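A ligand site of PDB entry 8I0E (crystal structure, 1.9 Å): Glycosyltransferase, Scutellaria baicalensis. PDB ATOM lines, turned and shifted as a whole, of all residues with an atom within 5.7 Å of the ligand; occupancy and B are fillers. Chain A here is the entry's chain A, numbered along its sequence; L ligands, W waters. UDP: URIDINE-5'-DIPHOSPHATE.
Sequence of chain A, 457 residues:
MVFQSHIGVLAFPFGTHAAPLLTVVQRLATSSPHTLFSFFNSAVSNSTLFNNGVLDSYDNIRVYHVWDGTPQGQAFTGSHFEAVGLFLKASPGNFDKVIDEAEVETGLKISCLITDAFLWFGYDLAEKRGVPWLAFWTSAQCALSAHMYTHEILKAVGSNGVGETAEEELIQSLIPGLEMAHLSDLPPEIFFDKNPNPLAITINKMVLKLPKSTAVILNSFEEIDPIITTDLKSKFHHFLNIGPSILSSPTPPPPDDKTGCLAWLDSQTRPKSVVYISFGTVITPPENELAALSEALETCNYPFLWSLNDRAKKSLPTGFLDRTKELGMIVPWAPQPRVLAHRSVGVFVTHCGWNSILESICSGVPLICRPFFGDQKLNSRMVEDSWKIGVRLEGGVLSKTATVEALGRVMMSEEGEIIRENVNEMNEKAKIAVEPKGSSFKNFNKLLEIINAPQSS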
ATOM      1  N   GLY A  15     -19.969 -23.090   3.528  1.00  0.00           N
ATOM      2  CA  GLY A  15     -20.907 -24.045   2.923  1.00  0.00           C
ATOM      3  C   GLY A  15     -22.081 -23.288   2.335  1.00  0.00           C
ATOM      4  O   GLY A  15     -21.848 -22.245   1.691  1.00  0.00           O
ATOM      5  N   THR A  16     -23.299 -23.752   2.590  1.00  0.00           N
ATOM      6  CA  THR A  16     -24.531 -23.107   2.080  1.00  0.00           C
ATOM      7  C   THR A  16     -25.284 -22.570   3.292  1.00  0.00           C
ATOM      8  O   THR A  16     -26.487 -22.749   3.353  1.00  0.00           O
ATOM      9  CB  THR A  16     -25.297 -24.078   1.173  1.00  0.00           C
ATOM     10  OG1 THR A  16     -25.546 -25.253   1.942  1.00  0.00           O
ATOM     11  CG2 THR A  16     -24.523 -24.412  -0.078  1.00  0.00           C
ATOM     12  N   TYR A 276     -31.186 -36.198 -13.486  1.00  0.00           N
ATOM     13  CA  TYR A 276     -30.351 -35.045 -13.067  1.00  0.00           C
ATOM     14  C   TYR A 276     -29.387 -35.499 -11.959  1.00  0.00           C
ATOM     15  O   TYR A 276     -29.844 -36.144 -11.013  1.00  0.00           O
ATOM     16  CB  TYR A 276     -31.215 -33.870 -12.617  1.00  0.00           C
ATOM     17  CG  TYR A 276     -30.405 -32.727 -12.080  1.00  0.00           C
ATOM     18  CD1 TYR A 276     -29.495 -32.051 -12.877  1.00  0.00           C
ATOM     19  CD2 TYR A 276     -30.511 -32.346 -10.756  1.00  0.00           C
ATOM     20  CE1 TYR A 276     -28.740 -30.992 -12.388  1.00  0.00           C
ATOM     21  CE2 TYR A 276     -29.744 -31.308 -10.247  1.00  0.00           C
ATOM     22  CZ  TYR A 276     -28.853 -30.634 -11.059  1.00  0.00           C
ATOM     23  OH  TYR A 276     -28.116 -29.595 -10.544  1.00  0.00           O
ATOM     24  N   SER A 278     -26.160 -34.093  -9.341  1.00  0.00           N
ATOM     25  CA  SER A 278     -25.309 -33.035  -8.755  1.00  0.00           C
ATOM     26  C   SER A 278     -24.848 -33.427  -7.352  1.00  0.00           C
ATOM     27  O   SER A 278     -25.715 -33.695  -6.519  1.00  0.00           O
ATOM     28  CB  SER A 278     -26.079 -31.742  -8.701  1.00  0.00           C
ATOM     29  OG  SER A 278     -25.235 -30.703  -8.281  1.00  0.00           O
ATOM     30  N   GLY A 280     -23.314 -31.235  -5.579  1.00  0.00           N
ATOM     31  CA  GLY A 280     -23.023 -29.837  -5.195  1.00  0.00           C
ATOM     32  C   GLY A 280     -21.901 -29.265  -6.040  1.00  0.00           C
ATOM     33  O   GLY A 280     -21.488 -29.916  -7.007  1.00  0.00           O
ATOM     34  N   THR A 281     -21.380 -28.102  -5.660  1.00  0.00           N
ATOM     35  CA  THR A 281     -20.397 -27.313  -6.456  1.00  0.00           C
ATOM     36  C   THR A 281     -18.963 -27.804  -6.183  1.00  0.00           C
ATOM     37  O   THR A 281     -18.139 -27.684  -7.100  1.00  0.00           O
ATOM     38  CB  THR A 281     -20.623 -25.815  -6.193  1.00  0.00           C
ATOM     39  OG1 THR A 281     -20.582 -25.557  -4.785  1.00  0.00           O
ATOM     40  CG2 THR A 281     -21.962 -25.319  -6.697  1.00  0.00           C
ATOM     41  N   SER A 307     -24.324 -31.946 -13.477  1.00  0.00           N
ATOM     42  CA  SER A 307     -23.523 -30.789 -13.017  1.00  0.00           C
ATOM     43  C   SER A 307     -22.244 -31.333 -12.371  1.00  0.00           C
ATOM     44  O   SER A 307     -22.330 -31.931 -11.291  1.00  0.00           O
ATOM     45  CB  SER A 307     -24.315 -29.918 -12.073  1.00  0.00           C
ATOM     46  OG  SER A 307     -23.555 -28.799 -11.654  1.00  0.00           O
ATOM     47  N   PRO A 332     -20.496 -27.519 -15.941  1.00  0.00           N
ATOM     48  CA  PRO A 332     -19.846 -27.216 -14.662  1.00  0.00           C
ATOM     49  C   PRO A 332     -20.795 -26.606 -13.619  1.00  0.00           C
ATOM     50  O   PRO A 332     -20.443 -26.611 -12.474  1.00  0.00           O
ATOM     51  CB  PRO A 332     -18.784 -26.179 -15.047  1.00  0.00           C
ATOM     52  CG  PRO A 332     -19.425 -25.448 -16.209  1.00  0.00           C
ATOM     53  CD  PRO A 332     -20.092 -26.568 -16.995  1.00  0.00           C
ATOM     54  N   TRP A 333     -21.942 -26.071 -14.055  1.00  0.00           N
ATOM     55  CA  TRP A 333     -22.972 -25.462 -13.179  1.00  0.00           C
ATOM     56  C   TRP A 333     -24.332 -25.523 -13.893  1.00  0.00           C
ATOM     57  O   TRP A 333     -24.380 -25.242 -15.108  1.00  0.00           O
ATOM     58  CB  TRP A 333     -22.595 -24.025 -12.823  1.00  0.00           C
ATOM     59  CG  TRP A 333     -23.516 -23.382 -11.840  1.00  0.00           C
ATOM     60  CD1 TRP A 333     -23.389 -23.385 -10.481  1.00  0.00           C
ATOM     61  CD2 TRP A 333     -24.699 -22.609 -12.134  1.00  0.00           C
ATOM     62  NE1 TRP A 333     -24.417 -22.684  -9.909  1.00  0.00           N
ATOM     63  CE2 TRP A 333     -25.223 -22.188 -10.892  1.00  0.00           C
ATOM     64  CE3 TRP A 333     -25.361 -22.241 -13.312  1.00  0.00           C
ATOM     65  CZ2 TRP A 333     -26.386 -21.419 -10.808  1.00  0.00           C
ATOM     66  CZ3 TRP A 333     -26.513 -21.484 -13.229  1.00  0.00           C
ATOM     67  CH2 TRP A 333     -27.013 -21.081 -11.981  1.00  0.00           C
ATOM     68  N   ALA A 334     -25.394 -25.872 -13.148  1.00  0.00           N
ATOM     69  CA  ALA A 334     -26.791 -25.909 -13.618  1.00  0.00           C
ATOM     70  C   ALA A 334     -27.612 -24.950 -12.786  1.00  0.00           C
ATOM     71  O   ALA A 334     -27.347 -24.744 -11.604  1.00  0.00           O
ATOM     72  CB  ALA A 334     -27.341 -27.309 -13.535  1.00  0.00           C
ATOM     73  N   PRO A 335     -28.672 -24.342 -13.351  1.00  0.00           N
ATOM     74  CA  PRO A 335     -29.629 -23.599 -12.543  1.00  0.00           C
ATOM     75  C   PRO A 335     -30.555 -24.630 -11.881  1.00  0.00           C
ATOM     76  O   PRO A 335     -31.643 -24.887 -12.366  1.00  0.00           O
ATOM     77  CB  PRO A 335     -30.300 -22.665 -13.561  1.00  0.00           C
ATOM     78  CG  PRO A 335     -30.226 -23.421 -14.867  1.00  0.00           C
ATOM     79  CD  PRO A 335     -28.984 -24.297 -14.790  1.00  0.00           C
ATOM     80  N   GLN A 336     -30.076 -25.222 -10.780  1.00  0.00           N
ATOM     81  CA  GLN A 336     -30.636 -26.476 -10.223  1.00  0.00           C
ATOM     82  C   GLN A 336     -32.142 -26.334 -10.006  1.00  0.00           C
ATOM     83  O   GLN A 336     -32.882 -27.197 -10.429  1.00  0.00           O
ATOM     84  CB  GLN A 336     -29.943 -26.880  -8.935  1.00  0.00           C
ATOM     85  CG  GLN A 336     -30.517 -28.180  -8.370  1.00  0.00           C
ATOM     86  CD  GLN A 336     -29.562 -28.835  -7.415  1.00  0.00           C
ATOM     87  OE1 GLN A 336     -28.489 -29.320  -7.789  1.00  0.00           O
ATOM     88  NE2 GLN A 336     -29.921 -28.750  -6.150  1.00  0.00           N
ATOM     89  N   PRO A 337     -32.654 -25.286  -9.316  1.00  0.00           N
ATOM     90  CA  PRO A 337     -34.083 -25.213  -9.018  1.00  0.00           C
ATOM     91  C   PRO A 337     -34.938 -25.190 -10.295  1.00  0.00           C
ATOM     92  O   PRO A 337     -35.986 -25.790 -10.313  1.00  0.00           O
ATOM     93  CB  PRO A 337     -34.248 -23.911  -8.206  1.00  0.00           C
ATOM     94  CG  PRO A 337     -32.854 -23.605  -7.704  1.00  0.00           C
ATOM     95  CD  PRO A 337     -31.907 -24.143  -8.752  1.00  0.00           C
ATOM     96  N   HIS A 351     -26.303 -35.437  -3.342  1.00  0.00           N
ATOM     97  CA  HIS A 351     -25.464 -35.592  -2.132  1.00  0.00           C
ATOM     98  C   HIS A 351     -26.320 -35.454  -0.858  1.00  0.00           C
ATOM     99  O   HIS A 351     -25.772 -35.653   0.243  1.00  0.00           O
ATOM    100  CB  HIS A 351     -24.255 -34.649  -2.174  1.00  0.00           C
ATOM    101  CG  HIS A 351     -24.560 -33.219  -1.936  1.00  0.00           C
ATOM    102  ND1 HIS A 351     -25.563 -32.555  -2.600  1.00  0.00           N
ATOM    103  CD2 HIS A 351     -23.962 -32.291  -1.155  1.00  0.00           C
ATOM    104  CE1 HIS A 351     -25.594 -31.298  -2.216  1.00  0.00           C
ATOM    105  NE2 HIS A 351     -24.629 -31.114  -1.324  1.00  0.00           N
ATOM    106  N   CYS A 352     -27.604 -35.120  -0.994  1.00  0.00           N
ATOM    107  CA  CYS A 352     -28.588 -35.065   0.116  1.00  0.00           C
ATOM    108  C   CYS A 352     -28.329 -33.846   1.019  1.00  0.00           C
ATOM    109  O   CYS A 352     -28.755 -33.865   2.148  1.00  0.00           O
ATOM    110  CB  CYS A 352     -28.538 -36.308   0.981  1.00  0.00           C
ATOM    111  SG  CYS A 352     -28.798 -37.824   0.028  1.00  0.00           S
ATOM    112  N   GLY A 353     -27.684 -32.823   0.517  1.00  0.00           N
ATOM    113  CA  GLY A 353     -27.750 -31.507   1.156  1.00  0.00           C
ATOM    114  C   GLY A 353     -29.196 -31.099   1.343  1.00  0.00           C
ATOM    115  O   GLY A 353     -30.000 -31.401   0.458  1.00  0.00           O
ATOM    116  N   TRP A 354     -29.521 -30.412   2.439  1.00  0.00           N
ATOM    117  CA  TRP A 354     -30.926 -30.049   2.758  1.00  0.00           C
ATOM    118  C   TRP A 354     -31.507 -29.150   1.668  1.00  0.00           C
ATOM    119  O   TRP A 354     -32.668 -29.367   1.292  1.00  0.00           O
ATOM    120  CB  TRP A 354     -31.019 -29.391   4.137  1.00  0.00           C
ATOM    121  CG  TRP A 354     -32.381 -28.842   4.408  1.00  0.00           C
ATOM    122  CD1 TRP A 354     -32.716 -27.550   4.671  1.00  0.00           C
ATOM    123  CD2 TRP A 354     -33.620 -29.581   4.388  1.00  0.00           C
ATOM    124  NE1 TRP A 354     -34.065 -27.438   4.876  1.00  0.00           N
ATOM    125  CE2 TRP A 354     -34.648 -28.662   4.687  1.00  0.00           C
ATOM    126  CE3 TRP A 354     -33.960 -30.928   4.186  1.00  0.00           C
ATOM    127  CZ2 TRP A 354     -35.980 -29.046   4.769  1.00  0.00           C
ATOM    128  CZ3 TRP A 354     -35.283 -31.303   4.262  1.00  0.00           C
ATOM    129  CH2 TRP A 354     -36.280 -30.376   4.535  1.00  0.00           C
ATOM    130  N   ASN A 355     -30.762 -28.172   1.142  1.00  0.00           N
ATOM    131  CA  ASN A 355     -31.321 -27.241   0.121  1.00  0.00           C
ATOM    132  C   ASN A 355     -31.723 -28.027  -1.121  1.00  0.00           C
ATOM    133  O   ASN A 355     -32.795 -27.726  -1.667  1.00  0.00           O
ATOM    134  CB  ASN A 355     -30.366 -26.116  -0.251  1.00  0.00           C
ATOM    135  CG  ASN A 355     -30.156 -25.181   0.916  1.00  0.00           C
ATOM    136  OD1 ASN A 355     -31.092 -24.498   1.341  1.00  0.00           O
ATOM    137  ND2 ASN A 355     -28.962 -25.174   1.475  1.00  0.00           N
ATOM    138  N   SER A 356     -30.860 -28.942  -1.569  1.00  0.00           N
ATOM    139  CA  SER A 356     -31.082 -29.791  -2.754  1.00  0.00           C
ATOM    140  C   SER A 356     -32.312 -30.669  -2.549  1.00  0.00           C
ATOM    141  O   SER A 356     -33.171 -30.692  -3.432  1.00  0.00           O
ATOM    142  CB  SER A 356     -29.857 -30.621  -3.036  1.00  0.00           C
ATOM    143  OG  SER A 356     -28.886 -29.774  -3.597  1.00  0.00           O
ATOM    144  N   ILE A 357     -32.427 -31.304  -1.382  1.00  0.00           N
ATOM    145  CA  ILE A 357     -33.606 -32.167  -1.051  1.00  0.00           C
ATOM    146  C   ILE A 357     -34.881 -31.295  -1.080  1.00  0.00           C
ATOM    147  O   ILE A 357     -35.872 -31.733  -1.676  1.00  0.00           O
ATOM    148  CB  ILE A 357     -33.420 -32.851   0.299  1.00  0.00           C
ATOM    149  CG1 ILE A 357     -32.410 -33.983   0.202  1.00  0.00           C
ATOM    150  CG2 ILE A 357     -34.752 -33.329   0.826  1.00  0.00           C
ATOM    151  CD1 ILE A 357     -31.956 -34.498   1.532  1.00  0.00           C
ATOM    152  N   GLU A 359     -35.493 -28.458  -2.639  1.00  0.00           N
ATOM    153  CA  GLU A 359     -35.758 -28.084  -4.044  1.00  0.00           C
ATOM    154  C   GLU A 359     -36.399 -29.274  -4.744  1.00  0.00           C
ATOM    155  O   GLU A 359     -37.363 -29.068  -5.504  1.00  0.00           O
ATOM    156  CB  GLU A 359     -34.471 -27.647  -4.727  1.00  0.00           C
ATOM    157  CG  GLU A 359     -33.998 -26.278  -4.261  1.00  0.00           C
ATOM    158  CD  GLU A 359     -32.556 -25.974  -4.620  1.00  0.00           C
ATOM    159  OE1 GLU A 359     -31.936 -26.801  -5.322  1.00  0.00           O
ATOM    160  OE2 GLU A 359     -32.040 -24.920  -4.182  1.00  0.00           O
ATOM    161  N   PHE A 373     -21.277 -36.087   3.980  1.00  0.00           N
ATOM    162  CA  PHE A 373     -20.863 -35.598   5.315  1.00  0.00           C
ATOM    163  C   PHE A 373     -21.996 -34.866   6.023  1.00  0.00           C
ATOM    164  O   PHE A 373     -23.003 -34.493   5.381  1.00  0.00           O
ATOM    165  CB  PHE A 373     -19.654 -34.680   5.177  1.00  0.00           C
ATOM    166  CG  PHE A 373     -19.933 -33.390   4.452  1.00  0.00           C
ATOM    167  CD1 PHE A 373     -20.490 -32.311   5.123  1.00  0.00           C
ATOM    168  CD2 PHE A 373     -19.644 -33.262   3.109  1.00  0.00           C
ATOM    169  CE1 PHE A 373     -20.755 -31.126   4.456  1.00  0.00           C
ATOM    170  CE2 PHE A 373     -19.891 -32.067   2.452  1.00  0.00           C
ATOM    171  CZ  PHE A 373     -20.455 -31.004   3.121  1.00  0.00           C
ATOM    172  N   ASP A 375     -25.057 -33.605   7.940  1.00  0.00           N
ATOM    173  CA  ASP A 375     -26.484 -33.979   8.049  1.00  0.00           C
ATOM    174  C   ASP A 375     -26.886 -34.832   6.834  1.00  0.00           C
ATOM    175  O   ASP A 375     -28.002 -35.336   6.832  1.00  0.00           O
ATOM    176  CB  ASP A 375     -27.362 -32.735   8.186  1.00  0.00           C
ATOM    177  CG  ASP A 375     -27.450 -31.925   6.897  1.00  0.00           C
ATOM    178  OD1 ASP A 375     -26.569 -32.113   6.038  1.00  0.00           O
ATOM    179  OD2 ASP A 375     -28.399 -31.145   6.755  1.00  0.00           O
ATOM    180  N   GLN A 376     -25.992 -34.998   5.857  1.00  0.00           N
ATOM    181  CA  GLN A 376     -26.380 -35.678   4.600  1.00  0.00           C
ATOM    182  C   GLN A 376     -26.800 -37.127   4.860  1.00  0.00           C
ATOM    183  O   GLN A 376     -27.756 -37.573   4.201  1.00  0.00           O
ATOM    184  CB  GLN A 376     -25.273 -35.570   3.564  1.00  0.00           C
ATOM    185  CG  GLN A 376     -25.093 -34.140   3.122  1.00  0.00           C
ATOM    186  CD  GLN A 376     -23.785 -33.893   2.423  1.00  0.00           C
ATOM    187  OE1 GLN A 376     -23.066 -34.817   2.033  1.00  0.00           O
ATOM    188  NE2 GLN A 376     -23.491 -32.624   2.229  1.00  0.00           N
HETATM  189  N1  UDP L   1     -26.519 -25.678  -6.903  1.00  0.00           N
HETATM  190  C2  UDP L   1     -26.735 -24.986  -8.111  1.00  0.00           C
HETATM  191  N3  UDP L   1     -26.167 -25.461  -9.251  1.00  0.00           N
HETATM  192  C4  UDP L   1     -25.372 -26.553  -9.266  1.00  0.00           C
HETATM  193  C5  UDP L   1     -25.125 -27.237  -8.084  1.00  0.00           C
HETATM  194  C6  UDP L   1     -25.733 -26.780  -6.898  1.00  0.00           C
HETATM  195  O2  UDP L   1     -27.496 -23.973  -8.118  1.00  0.00           O
HETATM  196  O4  UDP L   1     -24.851 -26.949 -10.349  1.00  0.00           O
HETATM  197  C1' UDP L   1     -27.128 -25.171  -5.654  1.00  0.00           C
HETATM  198  C2' UDP L   1     -28.394 -25.945  -5.280  1.00  0.00           C
HETATM  199  O2' UDP L   1     -29.566 -25.434  -5.919  1.00  0.00           O
HETATM  200  C3' UDP L   1     -28.448 -25.829  -3.765  1.00  0.00           C
HETATM  201  C4' UDP L   1     -26.988 -25.588  -3.354  1.00  0.00           C
HETATM  202  O4' UDP L   1     -26.219 -25.346  -4.543  1.00  0.00           O
HETATM  203  O3' UDP L   1     -29.258 -24.707  -3.405  1.00  0.00           O
HETATM  204  C5' UDP L   1     -26.392 -26.775  -2.625  1.00  0.00           C
HETATM  205  O5' UDP L   1     -26.986 -26.755  -1.327  1.00  0.00           O
HETATM  206  PA  UDP L   1     -27.159 -28.077  -0.415  1.00  0.00           P
HETATM  207  O1A UDP L   1     -27.713 -27.620   0.909  1.00  0.00           O
HETATM  208  O2A UDP L   1     -27.918 -29.155  -1.135  1.00  0.00           O
HETATM  209  O3A UDP L   1     -25.627 -28.664  -0.356  1.00  0.00           O
HETATM  210  PB  UDP L   1     -24.559 -28.478   0.860  1.00  0.00           P
HETATM  211  O1B UDP L   1     -25.359 -28.749   2.131  1.00  0.00           O
HETATM  212  O2B UDP L   1     -23.431 -29.473   0.613  1.00  0.00           O
HETATM  213  O3B UDP L   1     -24.173 -27.036   0.676  1.00  0.00           O
HETATM  214  O   HOH W   1     -29.931 -22.846  -6.122  1.00  0.00           O
HETATM  215  O   HOH W   2     -25.206 -30.560   3.702  1.00  0.00           O
HETATM  216  O   HOH W   3     -26.530 -29.795  -5.920  1.00  0.00           O
HETATM  217  O   HOH W   4     -29.445 -21.800  -8.915  1.00  0.00           O
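The side-chain hydroxyl of Thr 16 sits at hydrogen-bond distance from an oxygen (O3B) of the ligand (2.6 Å).
The side-chain hydroxyl (OG) of Ser 307 is in hydrogen-bond range of an oxygen (O4) of the ligand, 2.6 Å away.
N of Ser 356 sits at hydrogen-bond distance from O2A of the ligand.
OG of Ser 356 is in hydrogen-bond range of O2A of the ligand, 2.7 Å away.
An oxygen (O4) of the ligand lies within hydrogen-bond range of the backbone NH (N) of Ala 334.
A nitrogen (N3) of the ligand sits at hydrogen-bond distance from the backbone carbonyl oxygen of Ala 334.
The side-chain carboxylate (OE1) of Glu 359 sits at hydrogen-bond distance from an oxygen (O2') of the ligand (2.8 Å).
An oxygen (O1A) of the ligand is in hydrogen-bond range of the backbone NH (N) of Asn 355 (3.1 Å).
The side-chain amide nitrogen (ND2) of Asn 355 is in hydrogen-bond range of an oxygen (O1A) of the ligand (2.8 Å).
NE2 of His 351 sits at hydrogen-bond distance from O2B of the ligand (2.8 Å).
The side-chain amide nitrogen of Gln 336 lies close to an oxygen (O2') of the ligand (3.3 Å).
ND2 of Asn 355 is in hydrogen-bond range of OG1 of Thr 16, 3.4 Å away.
The side-chain hydroxyl (OG) of Ser 356 lies within hydrogen-bond range of the side-chain amide nitrogen (NE2) of Gln 336 (2.9 Å).
NE2 of Gln 336 sits at hydrogen-bond distance from OE1 of Glu 359, 2.9 Å away.
O of His 351 lies close to OE1 of Gln 376 (3.4 Å).
The side-chain amide oxygen (OE1) of Gln 336 lies within hydrogen-bond range of the side-chain hydroxyl (OH) of Tyr 276, at 2.8 Å.
The side-chain hydroxyl of Ser 278 lies close to the backbone NH of Gly 280.
OE1 of Gln 376 sits at hydrogen-bond distance from N of Phe 373 (2.9 Å).
NE1 of Trp 333 lies close to N3 of the ligand (3.3 Å).
The backbone carbonyl oxygen (O) of Gly 353 lies close to an oxygen (O2A) of the ligand, 3.5 Å away.
Ser 278 touches the ligand.
Thr 281 touches the ligand (CG2 to C5, 3.95 Å).
CD of Pro 337 touches O2' of the ligand (3.9 Å).
Trp 354 touches the ligand (N to O1A, 3.7 Å).
Gln 376 touches the ligand.
Hydrophobic or aromatic side chains that line the ligand: Trp 333, Pro 337 and His 351.
The nearest printed residue that does not touch the ligand is Phe 373 (4.2 Å).
Water W2 lies within hydrogen-bond range of an oxygen (O1B) of the ligand (2.4 Å), the side-chain amide nitrogen of Gln 376 (3.1 Å) and the side-chain carboxylate of Asp 375 (3.1 Å).
Water W3 lies within hydrogen-bond range of the side-chain amide oxygen (OE1) of Gln 336 (2.7 Å), the side-chain hydroxyl (OG) of Ser 278 (2.8 Å) and the side-chain hydroxyl (OG) of Ser 356 (3.3 Å).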
